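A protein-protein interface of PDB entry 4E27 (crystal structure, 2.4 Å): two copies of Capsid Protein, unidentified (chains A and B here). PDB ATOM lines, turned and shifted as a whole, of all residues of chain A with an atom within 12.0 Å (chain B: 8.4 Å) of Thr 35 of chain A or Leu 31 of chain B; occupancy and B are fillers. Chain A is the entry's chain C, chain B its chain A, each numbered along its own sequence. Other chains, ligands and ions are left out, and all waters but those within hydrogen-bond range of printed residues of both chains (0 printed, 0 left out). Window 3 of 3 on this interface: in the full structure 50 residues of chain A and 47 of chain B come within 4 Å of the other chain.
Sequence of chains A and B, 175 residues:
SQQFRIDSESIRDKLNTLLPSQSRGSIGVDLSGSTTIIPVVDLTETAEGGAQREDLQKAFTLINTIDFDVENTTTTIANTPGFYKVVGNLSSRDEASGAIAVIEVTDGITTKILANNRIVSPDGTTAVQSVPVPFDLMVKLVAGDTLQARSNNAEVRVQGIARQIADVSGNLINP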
ATOM      1  N   GLN A   2      16.777   1.526  -0.853  1.00  0.00           N
ATOM      2  CA  GLN A   2      16.969   1.663   0.587  1.00  0.00           C
ATOM      3  C   GLN A   2      16.938   3.122   0.985  1.00  0.00           C
ATOM      4  O   GLN A   2      17.083   4.005   0.145  1.00  0.00           O
ATOM      5  CB  GLN A   2      18.292   1.029   1.037  1.00  0.00           C
ATOM      6  N   GLN A   3      16.759   3.369   2.275  1.00  0.00           N
ATOM      7  CA  GLN A   3      16.633   4.725   2.781  1.00  0.00           C
ATOM      8  C   GLN A   3      17.702   4.977   3.843  1.00  0.00           C
ATOM      9  O   GLN A   3      18.256   4.034   4.405  1.00  0.00           O
ATOM     10  CB  GLN A   3      15.233   4.924   3.363  1.00  0.00           C
ATOM     11  CG  GLN A   3      14.769   6.367   3.422  1.00  0.00           C
ATOM     12  CD  GLN A   3      13.266   6.497   3.246  1.00  0.00           C
ATOM     13  OE1 GLN A   3      12.750   6.369   2.138  1.00  0.00           O
ATOM     14  NE2 GLN A   3      12.557   6.747   4.339  1.00  0.00           N
ATOM     15  N   PHE A   4      18.006   6.245   4.100  1.00  0.00           N
ATOM     16  CA  PHE A   4      18.940   6.601   5.164  1.00  0.00           C
ATOM     17  C   PHE A   4      18.608   7.980   5.720  1.00  0.00           C
ATOM     18  O   PHE A   4      18.277   8.900   4.970  1.00  0.00           O
ATOM     19  CB  PHE A   4      20.399   6.532   4.685  1.00  0.00           C
ATOM     20  CG  PHE A   4      20.792   7.642   3.741  1.00  0.00           C
ATOM     21  CD1 PHE A   4      20.633   7.494   2.376  1.00  0.00           C
ATOM     22  CD2 PHE A   4      21.337   8.826   4.222  1.00  0.00           C
ATOM     23  CE1 PHE A   4      20.997   8.506   1.508  1.00  0.00           C
ATOM     24  CE2 PHE A   4      21.702   9.841   3.359  1.00  0.00           C
ATOM     25  CZ  PHE A   4      21.529   9.681   1.997  1.00  0.00           C
ATOM     26  N   ARG A   5      18.698   8.120   7.038  1.00  0.00           N
ATOM     27  CA  ARG A   5      18.325   9.366   7.700  1.00  0.00           C
ATOM     28  C   ARG A   5      19.352  10.479   7.476  1.00  0.00           C
ATOM     29  O   ARG A   5      20.560  10.237   7.467  1.00  0.00           O
ATOM     30  CB  ARG A   5      18.111   9.130   9.198  1.00  0.00           C
ATOM     31  N   ILE A   6      18.860  11.699   7.291  1.00  0.00           N
ATOM     32  CA  ILE A   6      19.730  12.855   7.133  1.00  0.00           C
ATOM     33  C   ILE A   6      19.582  13.792   8.327  1.00  0.00           C
ATOM     34  O   ILE A   6      18.479  14.246   8.642  1.00  0.00           O
ATOM     35  CB  ILE A   6      19.418  13.631   5.836  1.00  0.00           C
ATOM     36  N   LEU A  31      13.208  13.597   7.754  1.00  0.00           N
ATOM     37  CA  LEU A  31      14.169  13.989   6.726  1.00  0.00           C
ATOM     38  C   LEU A  31      15.084  12.825   6.355  1.00  0.00           C
ATOM     39  O   LEU A  31      15.786  12.279   7.205  1.00  0.00           O
ATOM     40  CB  LEU A  31      15.000  15.189   7.193  1.00  0.00           C
ATOM     41  N   SER A  32      15.082  12.442   5.085  1.00  0.00           N
ATOM     42  CA  SER A  32      15.869  11.286   4.677  1.00  0.00           C
ATOM     43  C   SER A  32      16.440  11.388   3.263  1.00  0.00           C
ATOM     44  O   SER A  32      16.166  12.339   2.520  1.00  0.00           O
ATOM     45  CB  SER A  32      15.049   9.996   4.832  1.00  0.00           C
ATOM     46  OG  SER A  32      13.971   9.947   3.912  1.00  0.00           O
ATOM     47  N   GLY A  33      17.239  10.387   2.904  1.00  0.00           N
ATOM     48  CA  GLY A  33      17.867  10.332   1.599  1.00  0.00           C
ATOM     49  C   GLY A  33      17.731   8.972   0.944  1.00  0.00           C
ATOM     50  O   GLY A  33      17.394   7.982   1.593  1.00  0.00           O
ATOM     51  N   SER A  34      17.995   8.927  -0.355  1.00  0.00           N
ATOM     52  CA  SER A  34      17.915   7.684  -1.098  1.00  0.00           C
ATOM     53  C   SER A  34      19.302   7.251  -1.536  1.00  0.00           C
ATOM     54  O   SER A  34      20.222   8.059  -1.598  1.00  0.00           O
ATOM     55  CB  SER A  34      17.004   7.842  -2.310  1.00  0.00           C
ATOM     56  OG  SER A  34      16.953   6.649  -3.070  1.00  0.00           O
ATOM     57  N   THR A  35      19.444   5.961  -1.822  1.00  0.00           N
ATOM     58  CA  THR A  35      20.719   5.406  -2.253  1.00  0.00           C
ATOM     59  C   THR A  35      20.703   5.143  -3.752  1.00  0.00           C
ATOM     60  O   THR A  35      21.752   5.094  -4.395  1.00  0.00           O
ATOM     61  CB  THR A  35      21.045   4.095  -1.513  1.00  0.00           C
ATOM     62  OG1 THR A  35      19.946   3.184  -1.644  1.00  0.00           O
ATOM     63  CG2 THR A  35      21.302   4.366  -0.039  1.00  0.00           C
ATOM     64  N   THR A  36      19.506   4.975  -4.306  1.00  0.00           N
ATOM     65  CA  THR A  36      19.363   4.738  -5.736  1.00  0.00           C
ATOM     66  C   THR A  36      19.359   6.044  -6.517  1.00  0.00           C
ATOM     67  O   THR A  36      18.430   6.846  -6.403  1.00  0.00           O
ATOM     68  CB  THR A  36      18.075   3.970  -6.055  1.00  0.00           C
ATOM     69  N   ILE A  37      20.400   6.257  -7.314  1.00  0.00           N
ATOM     70  CA  ILE A  37      20.499   7.466  -8.124  1.00  0.00           C
ATOM     71  C   ILE A  37      19.594   7.380  -9.353  1.00  0.00           C
ATOM     72  O   ILE A  37      19.694   6.446 -10.146  1.00  0.00           O
ATOM     73  CB  ILE A  37      21.954   7.748  -8.543  1.00  0.00           C
ATOM     74  CG1 ILE A  37      22.843   7.852  -7.299  1.00  0.00           C
ATOM     75  CG2 ILE A  37      22.037   9.034  -9.361  1.00  0.00           C
ATOM     76  CD1 ILE A  37      24.322   7.728  -7.584  1.00  0.00           C
ATOM     77  N   ILE A  38      18.709   8.362  -9.502  1.00  0.00           N
ATOM     78  CA  ILE A  38      17.697   8.338 -10.557  1.00  0.00           C
ATOM     79  C   ILE A  38      18.096   9.187 -11.757  1.00  0.00           C
ATOM     80  O   ILE A  38      18.363  10.368 -11.616  1.00  0.00           O
ATOM     81  CB  ILE A  38      16.348   8.860 -10.027  1.00  0.00           C
ATOM     82  CG1 ILE A  38      15.943   8.103  -8.764  1.00  0.00           C
ATOM     83  CG2 ILE A  38      15.271   8.737 -11.087  1.00  0.00           C
ATOM     84  CD1 ILE A  38      15.899   6.603  -8.944  1.00  0.00           C
ATOM     85  N   PRO A  39      18.139   8.586 -12.955  1.00  0.00           N
ATOM     86  CA  PRO A  39      18.397   9.387 -14.160  1.00  0.00           C
ATOM     87  C   PRO A  39      17.140  10.143 -14.599  1.00  0.00           C
ATOM     88  O   PRO A  39      16.055   9.566 -14.586  1.00  0.00           O
ATOM     89  CB  PRO A  39      18.776   8.331 -15.196  1.00  0.00           C
ATOM     90  CG  PRO A  39      18.070   7.109 -14.750  1.00  0.00           C
ATOM     91  CD  PRO A  39      18.059   7.148 -13.247  1.00  0.00           C
ATOM     92  N   PHE B   4      20.367  -1.125 -10.394  1.00  0.00           N
ATOM     93  CA  PHE B   4      21.686  -1.758 -10.387  1.00  0.00           C
ATOM     94  C   PHE B   4      22.553  -1.137  -9.302  1.00  0.00           C
ATOM     95  O   PHE B   4      22.105  -0.244  -8.592  1.00  0.00           O
ATOM     96  CB  PHE B   4      22.369  -1.601 -11.747  1.00  0.00           C
ATOM     97  CG  PHE B   4      22.661  -0.174 -12.119  1.00  0.00           C
ATOM     98  CD1 PHE B   4      21.669   0.638 -12.647  1.00  0.00           C
ATOM     99  CD2 PHE B   4      23.930   0.356 -11.945  1.00  0.00           C
ATOM    100  CE1 PHE B   4      21.934   1.953 -12.991  1.00  0.00           C
ATOM    101  CE2 PHE B   4      24.202   1.672 -12.287  1.00  0.00           C
ATOM    102  CZ  PHE B   4      23.202   2.469 -12.811  1.00  0.00           C
ATOM    103  N   ARG B   5      23.793  -1.604  -9.177  1.00  0.00           N
ATOM    104  CA  ARG B   5      24.710  -1.072  -8.171  1.00  0.00           C
ATOM    105  C   ARG B   5      25.814  -0.222  -8.803  1.00  0.00           C
ATOM    106  O   ARG B   5      26.312  -0.546  -9.881  1.00  0.00           O
ATOM    107  CB  ARG B   5      25.322  -2.209  -7.347  1.00  0.00           C
ATOM    108  N   ILE B   6      26.194   0.863  -8.131  1.00  0.00           N
ATOM    109  CA  ILE B   6      27.197   1.786  -8.665  1.00  0.00           C
ATOM    110  C   ILE B   6      28.562   1.619  -8.003  1.00  0.00           C
ATOM    111  O   ILE B   6      28.651   1.363  -6.803  1.00  0.00           O
ATOM    112  CB  ILE B   6      26.754   3.260  -8.527  1.00  0.00           C
ATOM    113  N   ASP B   7      29.621   1.771  -8.797  1.00  0.00           N
ATOM    114  CA  ASP B   7      30.993   1.669  -8.306  1.00  0.00           C
ATOM    115  C   ASP B   7      31.765   2.961  -8.569  1.00  0.00           C
ATOM    116  O   ASP B   7      32.322   3.156  -9.651  1.00  0.00           O
ATOM    117  CB  ASP B   7      31.711   0.478  -8.951  1.00  0.00           C
ATOM    118  N   SER B   8      31.796   3.831  -7.563  1.00  0.00           N
ATOM    119  CA  SER B   8      32.457   5.130  -7.661  1.00  0.00           C
ATOM    120  C   SER B   8      32.599   5.720  -6.275  1.00  0.00           C
ATOM    121  O   SER B   8      31.609   5.916  -5.581  1.00  0.00           O
ATOM    122  CB  SER B   8      31.646   6.094  -8.530  1.00  0.00           C
ATOM    123  OG  SER B   8      32.214   7.396  -8.514  1.00  0.00           O
ATOM    124  N   ILE B  11      31.422   9.692  -6.014  1.00  0.00           N
ATOM    125  CA  ILE B  11      29.979   9.886  -5.894  1.00  0.00           C
ATOM    126  C   ILE B  11      29.465   9.544  -4.492  1.00  0.00           C
ATOM    127  O   ILE B  11      28.637  10.266  -3.929  1.00  0.00           O
ATOM    128  CB  ILE B  11      29.219   9.102  -6.982  1.00  0.00           C
ATOM    129  CG1 ILE B  11      29.546   9.685  -8.359  1.00  0.00           C
ATOM    130  CG2 ILE B  11      27.722   9.150  -6.744  1.00  0.00           C
ATOM    131  CD1 ILE B  11      28.864   8.987  -9.495  1.00  0.00           C
ATOM    132  N   ARG B  12      29.984   8.461  -3.916  1.00  0.00           N
ATOM    133  CA  ARG B  12      29.656   8.117  -2.534  1.00  0.00           C
ATOM    134  C   ARG B  12      30.134   9.213  -1.592  1.00  0.00           C
ATOM    135  O   ARG B  12      29.461   9.550  -0.620  1.00  0.00           O
ATOM    136  CB  ARG B  12      30.282   6.777  -2.146  1.00  0.00           C
ATOM    137  N   ASP B  13      31.294   9.792  -1.840  1.00  0.00           N
ATOM    138  CA  ASP B  13      31.738  10.923  -1.049  1.00  0.00           C
ATOM    139  C   ASP B  13      30.917  12.194  -1.272  1.00  0.00           C
ATOM    140  O   ASP B  13      30.589  12.851  -0.337  1.00  0.00           O
ATOM    141  CB  ASP B  13      33.227  11.214  -1.233  1.00  0.00           C
ATOM    142  N   LEU B  15      27.804  12.373  -2.095  1.00  0.00           N
ATOM    143  CA  LEU B  15      26.563  12.108  -1.420  1.00  0.00           C
ATOM    144  C   LEU B  15      26.683  12.069   0.086  1.00  0.00           C
ATOM    145  O   LEU B  15      25.746  12.328   0.784  1.00  0.00           O
ATOM    146  CB  LEU B  15      26.011  10.792  -1.918  1.00  0.00           C
ATOM    147  CG  LEU B  15      24.560  10.594  -1.648  1.00  0.00           C
ATOM    148  CD1 LEU B  15      23.870  11.748  -2.303  1.00  0.00           C
ATOM    149  CD2 LEU B  15      24.028   9.293  -2.176  1.00  0.00           C
ATOM    150  N   LEU B  31      25.302   1.708  -2.535  1.00  0.00           N
ATOM    151  CA  LEU B  31      24.690   2.732  -3.381  1.00  0.00           C
ATOM    152  C   LEU B  31      24.243   2.154  -4.721  1.00  0.00           C
ATOM    153  O   LEU B  31      24.979   1.410  -5.371  1.00  0.00           O
ATOM    154  CB  LEU B  31      25.645   3.911  -3.607  1.00  0.00           C
ATOM    155  N   SER B  32      23.035   2.519  -5.135  1.00  0.00           N
ATOM    156  CA  SER B  32      22.411   1.915  -6.299  1.00  0.00           C
ATOM    157  C   SER B  32      22.202   2.908  -7.446  1.00  0.00           C
ATOM    158  O   SER B  32      22.377   4.118  -7.285  1.00  0.00           O
ATOM    159  CB  SER B  32      21.069   1.309  -5.892  1.00  0.00           C
ATOM    160  OG  SER B  32      20.635   0.348  -6.830  1.00  0.00           O
ATOM    161  N   GLY B  33      21.828   2.379  -8.606  1.00  0.00           N
ATOM    162  CA  GLY B  33      21.457   3.198  -9.745  1.00  0.00           C
ATOM    163  C   GLY B  33      20.138   2.715 -10.319  1.00  0.00           C
ATOM    164  O   GLY B  33      19.677   1.620  -9.986  1.00  0.00           O
ATOM    165  N   SER B  34      19.522   3.523 -11.178  1.00  0.00           N
ATOM    166  CA  SER B  34      18.253   3.145 -11.796  1.00  0.00           C
ATOM    167  C   SER B  34      18.304   3.280 -13.308  1.00  0.00           C
ATOM    168  O   SER B  34      19.023   4.121 -13.844  1.00  0.00           O
ATOM    169  CB  SER B  34      17.102   3.983 -11.242  1.00  0.00           C
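7 positions are printed for both chains.
Of the 9 pairs that touch across the chains among the printed residues, none has its exchanged pair printed and touching as well.
The side-chain hydroxyl of Ser 8 of chain B sits at hydrogen-bond distance from the backbone NH of Ile 11 of chain B, 3.5 Å away.
The backbone carbonyl oxygen (O) of Phe 4 of chain B is in hydrogen-bond range of the backbone NH (N) of Gly 33 of chain B.
The backbone carbonyl oxygen (O) of Gln 2 of chain A is in hydrogen-bond range of the side-chain hydroxyl (OG1) of Thr 35 of chain A.
N of Thr 36 of chain A is in hydrogen-bond range of OG of Ser 34 of chain A (3.3 Å).
The backbone carbonyl oxygen of Leu 31 of chain B sits at hydrogen-bond distance from the backbone NH of Ile 6 of chain B, at 3.1 Å.
O of Ser 32 of chain B is in hydrogen-bond range of N of Ile 37 of chain A (2.9 Å).
The backbone NH of Ser 32 of chain B lies within hydrogen-bond range of the backbone carbonyl oxygen of Thr 35 of chain A, 3.0 Å away.
The backbone NH (N) of Ser 34 of chain B is in hydrogen-bond range of the backbone carbonyl oxygen (O) of Ile 37 of chain A (3.1 Å).
No residue of chain B comes within 4 Å of Gln 2 of chain A.
No residue of chain B comes within 4 Å of Ser 34 of chain A.
Thr 35 of chain A touches just these residues of chain B: Leu 31 (3.9 Å) and Ser 32 (3.0 Å).
Printed residues of chain B within 4 Å of Ile 37 of chain A: Ile 11, Ser 32, Gly 33 and Ser 34.
Of the printed residues of chain B, Pro 39 of chain A touches Ser 34.
No residue of chain A comes within 4 Å of Arg 5 of chain B.
No residue of chain A comes within 4 Å of Ile 6 of chain B.
No residue of chain A comes within 4 Å of Arg 12 of chain B.
Of the printed residues of chain A, Leu 31 of chain B touches Thr 35.
Gly 33 of chain B touches just one residue of chain A: Ile 37.
Of the printed residues of chain A, Ser 34 of chain B touches Ile 37 (3.1 Å), Ile 38 (3.7 Å) and Pro 39 (3.2 Å).
The nearest residue of chain B that does not touch Thr 35 of chain A is Gly 33 of chain B (5.0 Å).
The nearest residue of chain A that does not touch Leu 31 of chain B is Thr 36 of chain A (5.5 Å).
The nearest printed residue of chain B that does not touch Pro 39 of chain A is Gly 33 of chain B (5.7 Å).
Among the printed residues, pairs that only touch across the chains: Thr 35 of chain A with Leu 31 of chain B (3.9 Å), Thr 36 of chain A with Ser 32 of chain B (3.4 Å), Ile 37 of chain A with Ile 11 of chain B (3.8 Å), Ile 37 of chain A with Gly 33 of chain B (3.7 Å), Ile 38 of chain A with Ser 34 of chain B (3.7 Å) and Pro 39 of chain A with Ser 34 of chain B (3.2 Å).
Printed residues of chain A that touch a printed residue of chain B: Thr 35, Thr 36, Ile 37, Ile 38 and Pro 39.
Of the 13 printed residues of chain B, 5 touch a printed residue of chain A.
Among the printed residues, no Asp or Glu carboxylate lies within 4 Å of a Lys or Arg side-chain nitrogen of the other chain.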
